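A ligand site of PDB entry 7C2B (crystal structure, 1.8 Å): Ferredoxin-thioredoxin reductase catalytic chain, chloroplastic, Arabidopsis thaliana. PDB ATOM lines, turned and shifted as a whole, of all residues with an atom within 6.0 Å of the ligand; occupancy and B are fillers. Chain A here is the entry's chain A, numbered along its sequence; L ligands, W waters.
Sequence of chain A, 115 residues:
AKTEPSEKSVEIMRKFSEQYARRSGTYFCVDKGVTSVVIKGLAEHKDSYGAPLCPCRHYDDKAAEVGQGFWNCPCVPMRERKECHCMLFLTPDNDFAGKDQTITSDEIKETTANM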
ATOM      1  N   PHE A  16     -18.418  14.483  -1.471  1.00  0.00           N
ATOM      2  CA  PHE A  16     -19.139  13.257  -1.797  1.00  0.00           C
ATOM      3  C   PHE A  16     -20.484  13.203  -1.062  1.00  0.00           C
ATOM      4  O   PHE A  16     -21.520  12.943  -1.667  1.00  0.00           O
ATOM      5  CB  PHE A  16     -18.279  12.047  -1.442  1.00  0.00           C
ATOM      6  CG  PHE A  16     -19.069  10.803  -1.135  1.00  0.00           C
ATOM      7  CD1 PHE A  16     -19.925  10.247  -2.095  1.00  0.00           C
ATOM      8  CD2 PHE A  16     -18.965  10.184   0.100  1.00  0.00           C
ATOM      9  CE1 PHE A  16     -20.669   9.100  -1.817  1.00  0.00           C
ATOM     10  CE2 PHE A  16     -19.688   9.023   0.382  1.00  0.00           C
ATOM     11  CZ  PHE A  16     -20.550   8.479  -0.580  1.00  0.00           C
ATOM     12  N   VAL A  38     -18.960  10.471  10.852  1.00  0.00           N
ATOM     13  CA  VAL A  38     -18.907   9.456   9.808  1.00  0.00           C
ATOM     14  C   VAL A  38     -18.071   9.923   8.629  1.00  0.00           C
ATOM     15  O   VAL A  38     -17.291   9.159   8.044  1.00  0.00           O
ATOM     16  CB  VAL A  38     -20.334   9.071   9.378  1.00  0.00           C
ATOM     17  CG1 VAL A  38     -20.293   8.138   8.159  1.00  0.00           C
ATOM     18  CG2 VAL A  38     -21.066   8.396  10.577  1.00  0.00           C
ATOM     19  N   LEU A  42     -14.913   7.917   7.050  1.00  0.00           N
ATOM     20  CA  LEU A  42     -14.692   7.621   5.638  1.00  0.00           C
ATOM     21  C   LEU A  42     -13.333   8.143   5.193  1.00  0.00           C
ATOM     22  O   LEU A  42     -12.589   7.451   4.493  1.00  0.00           O
ATOM     23  CB  LEU A  42     -15.796   8.228   4.782  1.00  0.00           C
ATOM     24  CG  LEU A  42     -17.223   7.766   5.074  1.00  0.00           C
ATOM     25  CD1 LEU A  42     -18.229   8.580   4.242  1.00  0.00           C
ATOM     26  CD2 LEU A  42     -17.353   6.275   4.791  1.00  0.00           C
ATOM     27  N   PRO A  52     -12.867   4.415   1.225  1.00  0.00           N
ATOM     28  CA  PRO A  52     -13.722   4.756   2.385  1.00  0.00           C
ATOM     29  C   PRO A  52     -14.639   3.603   2.780  1.00  0.00           C
ATOM     30  O   PRO A  52     -15.861   3.618   2.566  1.00  0.00           O
ATOM     31  CB  PRO A  52     -14.509   5.974   1.876  1.00  0.00           C
ATOM     32  CG  PRO A  52     -14.614   5.738   0.416  1.00  0.00           C
ATOM     33  CD  PRO A  52     -13.297   5.134   0.011  1.00  0.00           C
ATOM     34  N   LEU A  53     -14.060   2.574   3.385  1.00  0.00           N
ATOM     35  CA  LEU A  53     -14.873   1.523   3.952  1.00  0.00           C
ATOM     36  C   LEU A  53     -15.766   2.098   5.041  1.00  0.00           C
ATOM     37  O   LEU A  53     -15.376   3.004   5.784  1.00  0.00           O
ATOM     38  CB  LEU A  53     -14.012   0.389   4.537  1.00  0.00           C
ATOM     39  CG  LEU A  53     -13.133  -0.368   3.556  1.00  0.00           C
ATOM     40  CD1 LEU A  53     -12.284  -1.387   4.284  1.00  0.00           C
ATOM     41  CD2 LEU A  53     -13.991  -1.039   2.496  1.00  0.00           C
ATOM     42  N   CYS A  54     -16.969   1.551   5.129  1.00  0.00           N
ATOM     43  CA  CYS A  54     -17.951   1.907   6.130  1.00  0.00           C
ATOM     44  C   CYS A  54     -17.296   1.970   7.512  1.00  0.00           C
ATOM     45  O   CYS A  54     -16.688   0.987   7.937  1.00  0.00           O
ATOM     46  CB  CYS A  54     -19.081   0.886   6.168  1.00  0.00           C
ATOM     47  SG  CYS A  54     -20.391   1.435   7.260  1.00  0.00           S
ATOM     48  N   PRO A  55     -17.387   3.100   8.217  1.00  0.00           N
ATOM     49  CA  PRO A  55     -16.806   3.162   9.565  1.00  0.00           C
ATOM     50  C   PRO A  55     -17.647   2.489  10.627  1.00  0.00           C
ATOM     51  O   PRO A  55     -17.207   2.414  11.783  1.00  0.00           O
ATOM     52  CB  PRO A  55     -16.695   4.675   9.839  1.00  0.00           C
ATOM     53  CG  PRO A  55     -17.700   5.310   8.960  1.00  0.00           C
ATOM     54  CD  PRO A  55     -17.864   4.414   7.739  1.00  0.00           C
ATOM     55  N   CYS A  56     -18.852   2.018  10.302  1.00  0.00           N
ATOM     56  CA  CYS A  56     -19.675   1.286  11.259  1.00  0.00           C
ATOM     57  C   CYS A  56     -19.722  -0.209  10.940  1.00  0.00           C
ATOM     58  O   CYS A  56     -20.737  -0.871  11.154  1.00  0.00           O
ATOM     59  CB  CYS A  56     -21.081   1.885  11.324  1.00  0.00           C
ATOM     60  SG  CYS A  56     -21.099   3.545  12.085  1.00  0.00           S
ATOM     61  N   TRP A  71     -18.585  -3.011   1.088  1.00  0.00           N
ATOM     62  CA  TRP A  71     -18.721  -2.061   2.177  1.00  0.00           C
ATOM     63  C   TRP A  71     -18.001  -0.744   1.897  1.00  0.00           C
ATOM     64  O   TRP A  71     -17.870   0.074   2.796  1.00  0.00           O
ATOM     65  CB  TRP A  71     -18.217  -2.654   3.487  1.00  0.00           C
ATOM     66  CG  TRP A  71     -19.162  -3.658   4.051  1.00  0.00           C
ATOM     67  CD1 TRP A  71     -18.904  -4.993   4.238  1.00  0.00           C
ATOM     68  CD2 TRP A  71     -20.505  -3.439   4.498  1.00  0.00           C
ATOM     69  NE1 TRP A  71     -20.010  -5.604   4.776  1.00  0.00           N
ATOM     70  CE2 TRP A  71     -21.018  -4.679   4.924  1.00  0.00           C
ATOM     71  CE3 TRP A  71     -21.336  -2.306   4.559  1.00  0.00           C
ATOM     72  CZ2 TRP A  71     -22.309  -4.822   5.427  1.00  0.00           C
ATOM     73  CZ3 TRP A  71     -22.631  -2.445   5.049  1.00  0.00           C
ATOM     74  CH2 TRP A  71     -23.110  -3.700   5.481  1.00  0.00           C
ATOM     75  N   ASN A  72     -17.499  -0.536   0.670  1.00  0.00           N
ATOM     76  CA  ASN A  72     -16.969   0.775   0.306  1.00  0.00           C
ATOM     77  C   ASN A  72     -18.098   1.768   0.136  1.00  0.00           C
ATOM     78  O   ASN A  72     -19.029   1.538  -0.638  1.00  0.00           O
ATOM     79  CB  ASN A  72     -16.155   0.697  -0.985  1.00  0.00           C
ATOM     80  CG  ASN A  72     -15.320   1.951  -1.205  1.00  0.00           C
ATOM     81  OD1 ASN A  72     -14.657   2.417  -0.289  1.00  0.00           O
ATOM     82  ND2 ASN A  72     -15.390   2.528  -2.403  1.00  0.00           N
ATOM     83  N   CYS A  73     -18.017   2.885   0.831  1.00  0.00           N
ATOM     84  CA  CYS A  73     -19.106   3.854   0.819  1.00  0.00           C
ATOM     85  C   CYS A  73     -19.195   4.535  -0.545  1.00  0.00           C
ATOM     86  O   CYS A  73     -18.160   4.955  -1.081  1.00  0.00           O
ATOM     87  CB  CYS A  73     -18.866   4.891   1.925  1.00  0.00           C
ATOM     88  SG  CYS A  73     -20.238   6.041   2.180  1.00  0.00           S
ATOM     89  N   PRO A  74     -20.383   4.644  -1.157  1.00  0.00           N
ATOM     90  CA  PRO A  74     -21.680   4.164  -0.676  1.00  0.00           C
ATOM     91  C   PRO A  74     -21.774   2.669  -0.809  1.00  0.00           C
ATOM     92  O   PRO A  74     -21.559   2.127  -1.898  1.00  0.00           O
ATOM     93  CB  PRO A  74     -22.696   4.851  -1.607  1.00  0.00           C
ATOM     94  CG  PRO A  74     -21.917   5.105  -2.893  1.00  0.00           C
ATOM     95  CD  PRO A  74     -20.466   5.269  -2.493  1.00  0.00           C
ATOM     96  N   CYS A  75     -22.085   2.003   0.302  1.00  0.00           N
ATOM     97  CA  CYS A  75     -22.063   0.543   0.323  1.00  0.00           C
ATOM     98  C   CYS A  75     -23.247  -0.046  -0.459  1.00  0.00           C
ATOM     99  O   CYS A  75     -24.190   0.649  -0.837  1.00  0.00           O
ATOM    100  CB  CYS A  75     -22.080   0.033   1.768  1.00  0.00           C
ATOM    101  SG  CYS A  75     -23.598   0.577   2.656  1.00  0.00           S
ATOM    102  N   VAL A  76     -23.209  -1.362  -0.677  1.00  0.00           N
ATOM    103  CA  VAL A  76     -24.292  -2.013  -1.400  1.00  0.00           C
ATOM    104  C   VAL A  76     -25.644  -1.804  -0.739  1.00  0.00           C
ATOM    105  O   VAL A  76     -26.617  -1.512  -1.460  1.00  0.00           O
ATOM    106  CB  VAL A  76     -23.956  -3.496  -1.632  1.00  0.00           C
ATOM    107  CG1 VAL A  76     -25.203  -4.253  -2.004  1.00  0.00           C
ATOM    108  CG2 VAL A  76     -22.920  -3.603  -2.745  1.00  0.00           C
ATOM    109  N   PRO A  77     -25.797  -1.936   0.584  1.00  0.00           N
ATOM    110  CA  PRO A  77     -27.135  -1.691   1.164  1.00  0.00           C
ATOM    111  C   PRO A  77     -27.644  -0.286   0.909  1.00  0.00           C
ATOM    112  O   PRO A  77     -28.853  -0.110   0.740  1.00  0.00           O
ATOM    113  CB  PRO A  77     -26.930  -1.961   2.672  1.00  0.00           C
ATOM    114  CG  PRO A  77     -25.868  -3.030   2.679  1.00  0.00           C
ATOM    115  CD  PRO A  77     -24.915  -2.602   1.560  1.00  0.00           C
ATOM    116  N   MET A  78     -26.761   0.715   0.886  1.00  0.00           N
ATOM    117  CA  MET A  78     -27.179   2.069   0.571  1.00  0.00           C
ATOM    118  C   MET A  78     -27.549   2.201  -0.906  1.00  0.00           C
ATOM    119  O   MET A  78     -28.602   2.730  -1.243  1.00  0.00           O
ATOM    120  CB  MET A  78     -26.074   3.058   0.946  1.00  0.00           C
ATOM    121  CG  MET A  78     -26.421   4.520   0.588  1.00  0.00           C
ATOM    122  SD  MET A  78     -27.860   5.041   1.564  1.00  0.00           S
ATOM    123  CE  MET A  78     -28.346   6.481   0.604  1.00  0.00           C
ATOM    124  N   GLU A  83     -30.252   1.950   2.615  1.00  0.00           N
ATOM    125  CA  GLU A  83     -30.043   1.638   4.021  1.00  0.00           C
ATOM    126  C   GLU A  83     -28.649   2.090   4.413  1.00  0.00           C
ATOM    127  O   GLU A  83     -27.650   1.524   3.951  1.00  0.00           O
ATOM    128  CB  GLU A  83     -30.227   0.139   4.273  1.00  0.00           C
ATOM    129  CG  GLU A  83     -31.672  -0.279   4.158  1.00  0.00           C
ATOM    130  CD  GLU A  83     -31.860  -1.775   4.381  1.00  0.00           C
ATOM    131  OE1 GLU A  83     -30.853  -2.490   4.600  1.00  0.00           O
ATOM    132  OE2 GLU A  83     -33.021  -2.233   4.312  1.00  0.00           O
ATOM    133  N   CYS A  84     -28.570   3.099   5.283  1.00  0.00           N
ATOM    134  CA  CYS A  84     -27.304   3.643   5.764  1.00  0.00           C
ATOM    135  C   CYS A  84     -27.283   3.514   7.280  1.00  0.00           C
ATOM    136  O   CYS A  84     -27.784   4.393   7.978  1.00  0.00           O
ATOM    137  CB  CYS A  84     -27.126   5.109   5.337  1.00  0.00           C
ATOM    138  SG  CYS A  84     -25.624   5.890   5.947  1.00  0.00           S
ATOM    139  N   HIS A  85     -26.682   2.430   7.803  1.00  0.00           N
ATOM    140  CA  HIS A  85     -26.728   2.239   9.255  1.00  0.00           C
ATOM    141  C   HIS A  85     -25.769   3.170   9.981  1.00  0.00           C
ATOM    142  O   HIS A  85     -25.901   3.326  11.203  1.00  0.00           O
ATOM    143  CB  HIS A  85     -26.466   0.759   9.602  1.00  0.00           C
ATOM    144  CG  HIS A  85     -25.053   0.315   9.359  1.00  0.00           C
ATOM    145  ND1 HIS A  85     -24.557   0.058   8.093  1.00  0.00           N
ATOM    146  CD2 HIS A  85     -24.030   0.095  10.218  1.00  0.00           C
ATOM    147  CE1 HIS A  85     -23.284  -0.278   8.187  1.00  0.00           C
ATOM    148  NE2 HIS A  85     -22.933  -0.271   9.460  1.00  0.00           N
ATOM    149  N   CYS A  86     -24.843   3.824   9.276  1.00  0.00           N
ATOM    150  CA  CYS A  86     -24.004   4.867   9.839  1.00  0.00           C
ATOM    151  C   CYS A  86     -24.777   6.139  10.175  1.00  0.00           C
ATOM    152  O   CYS A  86     -24.221   6.993  10.874  1.00  0.00           O
ATOM    153  CB  CYS A  86     -22.881   5.235   8.863  1.00  0.00           C
ATOM    154  SG  CYS A  86     -21.661   3.936   8.695  1.00  0.00           S
ATOM    155  N   MET A  87     -25.989   6.287   9.657  1.00  0.00           N
ATOM    156  CA  MET A  87     -26.804   7.508   9.803  1.00  0.00           C
ATOM    157  C   MET A  87     -26.144   8.709   9.130  1.00  0.00           C
ATOM    158  O   MET A  87     -26.310   9.857   9.562  1.00  0.00           O
ATOM    159  CB  MET A  87     -27.121   7.782  11.279  1.00  0.00           C
ATOM    160  CG  MET A  87     -27.769   6.566  11.919  1.00  0.00           C
ATOM    161  SD  MET A  87     -28.290   6.849  13.623  1.00  0.00           S
ATOM    162  CE  MET A  87     -26.890   7.714  14.285  1.00  0.00           C
ATOM    163  N   LEU A  88     -25.404   8.443   8.056  1.00  0.00           N
ATOM    164  CA  LEU A  88     -24.919   9.504   7.180  1.00  0.00           C
ATOM    165  C   LEU A  88     -26.011   9.979   6.222  1.00  0.00           C
ATOM    166  O   LEU A  88     -26.344  11.163   6.185  1.00  0.00           O
ATOM    167  CB  LEU A  88     -23.679   9.033   6.420  1.00  0.00           C
ATOM    168  CG  LEU A  88     -23.119   9.973   5.357  1.00  0.00           C
ATOM    169  CD1 LEU A  88     -22.889  11.352   5.946  1.00  0.00           C
ATOM    170  CD2 LEU A  88     -21.812   9.407   4.786  1.00  0.00           C
ATOM    171  N   PHE A  89     -26.614   9.047   5.463  1.00  0.00           N
ATOM    172  CA  PHE A  89     -27.675   9.331   4.497  1.00  0.00           C
ATOM    173  C   PHE A  89     -28.997   8.806   5.029  1.00  0.00           C
ATOM    174  O   PHE A  89     -29.203   7.594   5.070  1.00  0.00           O
ATOM    175  CB  PHE A  89     -27.366   8.683   3.146  1.00  0.00           C
ATOM    176  CG  PHE A  89     -26.032   9.038   2.596  1.00  0.00           C
ATOM    177  CD1 PHE A  89     -25.772  10.330   2.161  1.00  0.00           C
ATOM    178  CD2 PHE A  89     -25.030   8.082   2.472  1.00  0.00           C
ATOM    179  CE1 PHE A  89     -24.538  10.666   1.645  1.00  0.00           C
ATOM    180  CE2 PHE A  89     -23.772   8.427   1.941  1.00  0.00           C
ATOM    181  CZ  PHE A  89     -23.543   9.731   1.531  1.00  0.00           C
HETATM  182 FE1  LIG L   1     -21.550   4.768   3.643  1.00  0.00          FE
HETATM  183 FE2  LIG L   1     -21.635   3.266   6.133  1.00  0.00          FE
HETATM  184 FE3  LIG L   1     -22.920   2.484   3.831  1.00  0.00          FE
HETATM  185 FE4  LIG L   1     -23.750   4.684   5.145  1.00  0.00          FE
HETATM  186  S1  LIG L   1     -23.765   2.554   5.959  1.00  0.00           S
HETATM  187  S2  LIG L   1     -23.590   4.443   2.870  1.00  0.00           S
HETATM  188  S3  LIG L   1     -21.788   5.536   5.773  1.00  0.00           S
HETATM  189  S4  LIG L   1     -20.721   2.712   4.090  1.00  0.00           S
HETATM  190  O   HOH W   1     -26.097   0.034   5.900  1.00  0.00           O
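The side-chain sulfur (SG) of Cys 86 is bound to an iron atom (FE2) of the ligand.
An iron atom (FE3) of the ligand is bound by the side-chain sulfur of Cys 75 (2.3 Å).
The backbone NH (N) of Cys 86 sits close to a sulfur (S1) of the ligand, at 3.7 Å.
An iron atom (FE2) of the ligand is bound by the side-chain sulfur (SG) of Cys 54, at 2.5 Å.
The backbone NH (N) of His 85 sits close to a sulfur (S1) of the ligand (3.5 Å).
SG of Cys 84 is bound to FE4 of the ligand, at 2.4 Å.
A ring nitrogen (ND1) of His 85 lies close to a sulfur (S1) of the ligand (3.4 Å).
The side-chain sulfur (SG) of Cys 73 is bound to an iron atom (FE1) of the ligand (2.3 Å).
The side-chain sulfur (SG) of Cys 86 sits close to the side-chain sulfur (SG) of Cys 56, at 3.5 Å.
The backbone NH of Cys 73 sits at hydrogen-bond distance from the backbone carbonyl oxygen of Pro 52 (2.9 Å).
The side-chain sulfur (SG) of Cys 84 sits close to the backbone NH (N) of Leu 88 (3.3 Å).
The side-chain sulfur (SG) of Cys 84 sits close to the backbone NH (N) of Phe 89 (3.3 Å).
The backbone NH (N) of Met 87 sits close to the side-chain sulfur (SG) of Cys 84, 3.7 Å away.
The backbone NH (N) of Cys 54 is in hydrogen-bond range of the backbone carbonyl oxygen (O) of Trp 71.
SG of Cys 54 sits close to NE2 of His 85 (3.8 Å).
The side-chain sulfur (SG) of Cys 75 lies close to the backbone NH (N) of Met 78, at 3.6 Å.
Merely in contact with the ligand: Met 78 (3.4 Å), Val 38 (3.8 Å), Phe 89 (3.9 Å) and Leu 88 (3.99 Å).
Hydrophobic or aromatic side chains within 4 Å of the ligand: Val 38, Met 78, His 85, Leu 88 and Phe 89.
Within 4 Å of the ligand: Val 38, Cys 54, Cys 73, Cys 75, Met 78, Cys 84, His 85, Cys 86, Leu 88 and Phe 89.
Along chain A the residues within 4 Å of the ligand span positions 38 to 89.
The nearest printed residue that does not touch the ligand is Pro 74 (4.04 Å).
Water W1 lies within hydrogen-bond range of ND1 of His 85 (2.7 Å), O of Glu 83 (2.9 Å) and S1 of the ligand (3.4 Å).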
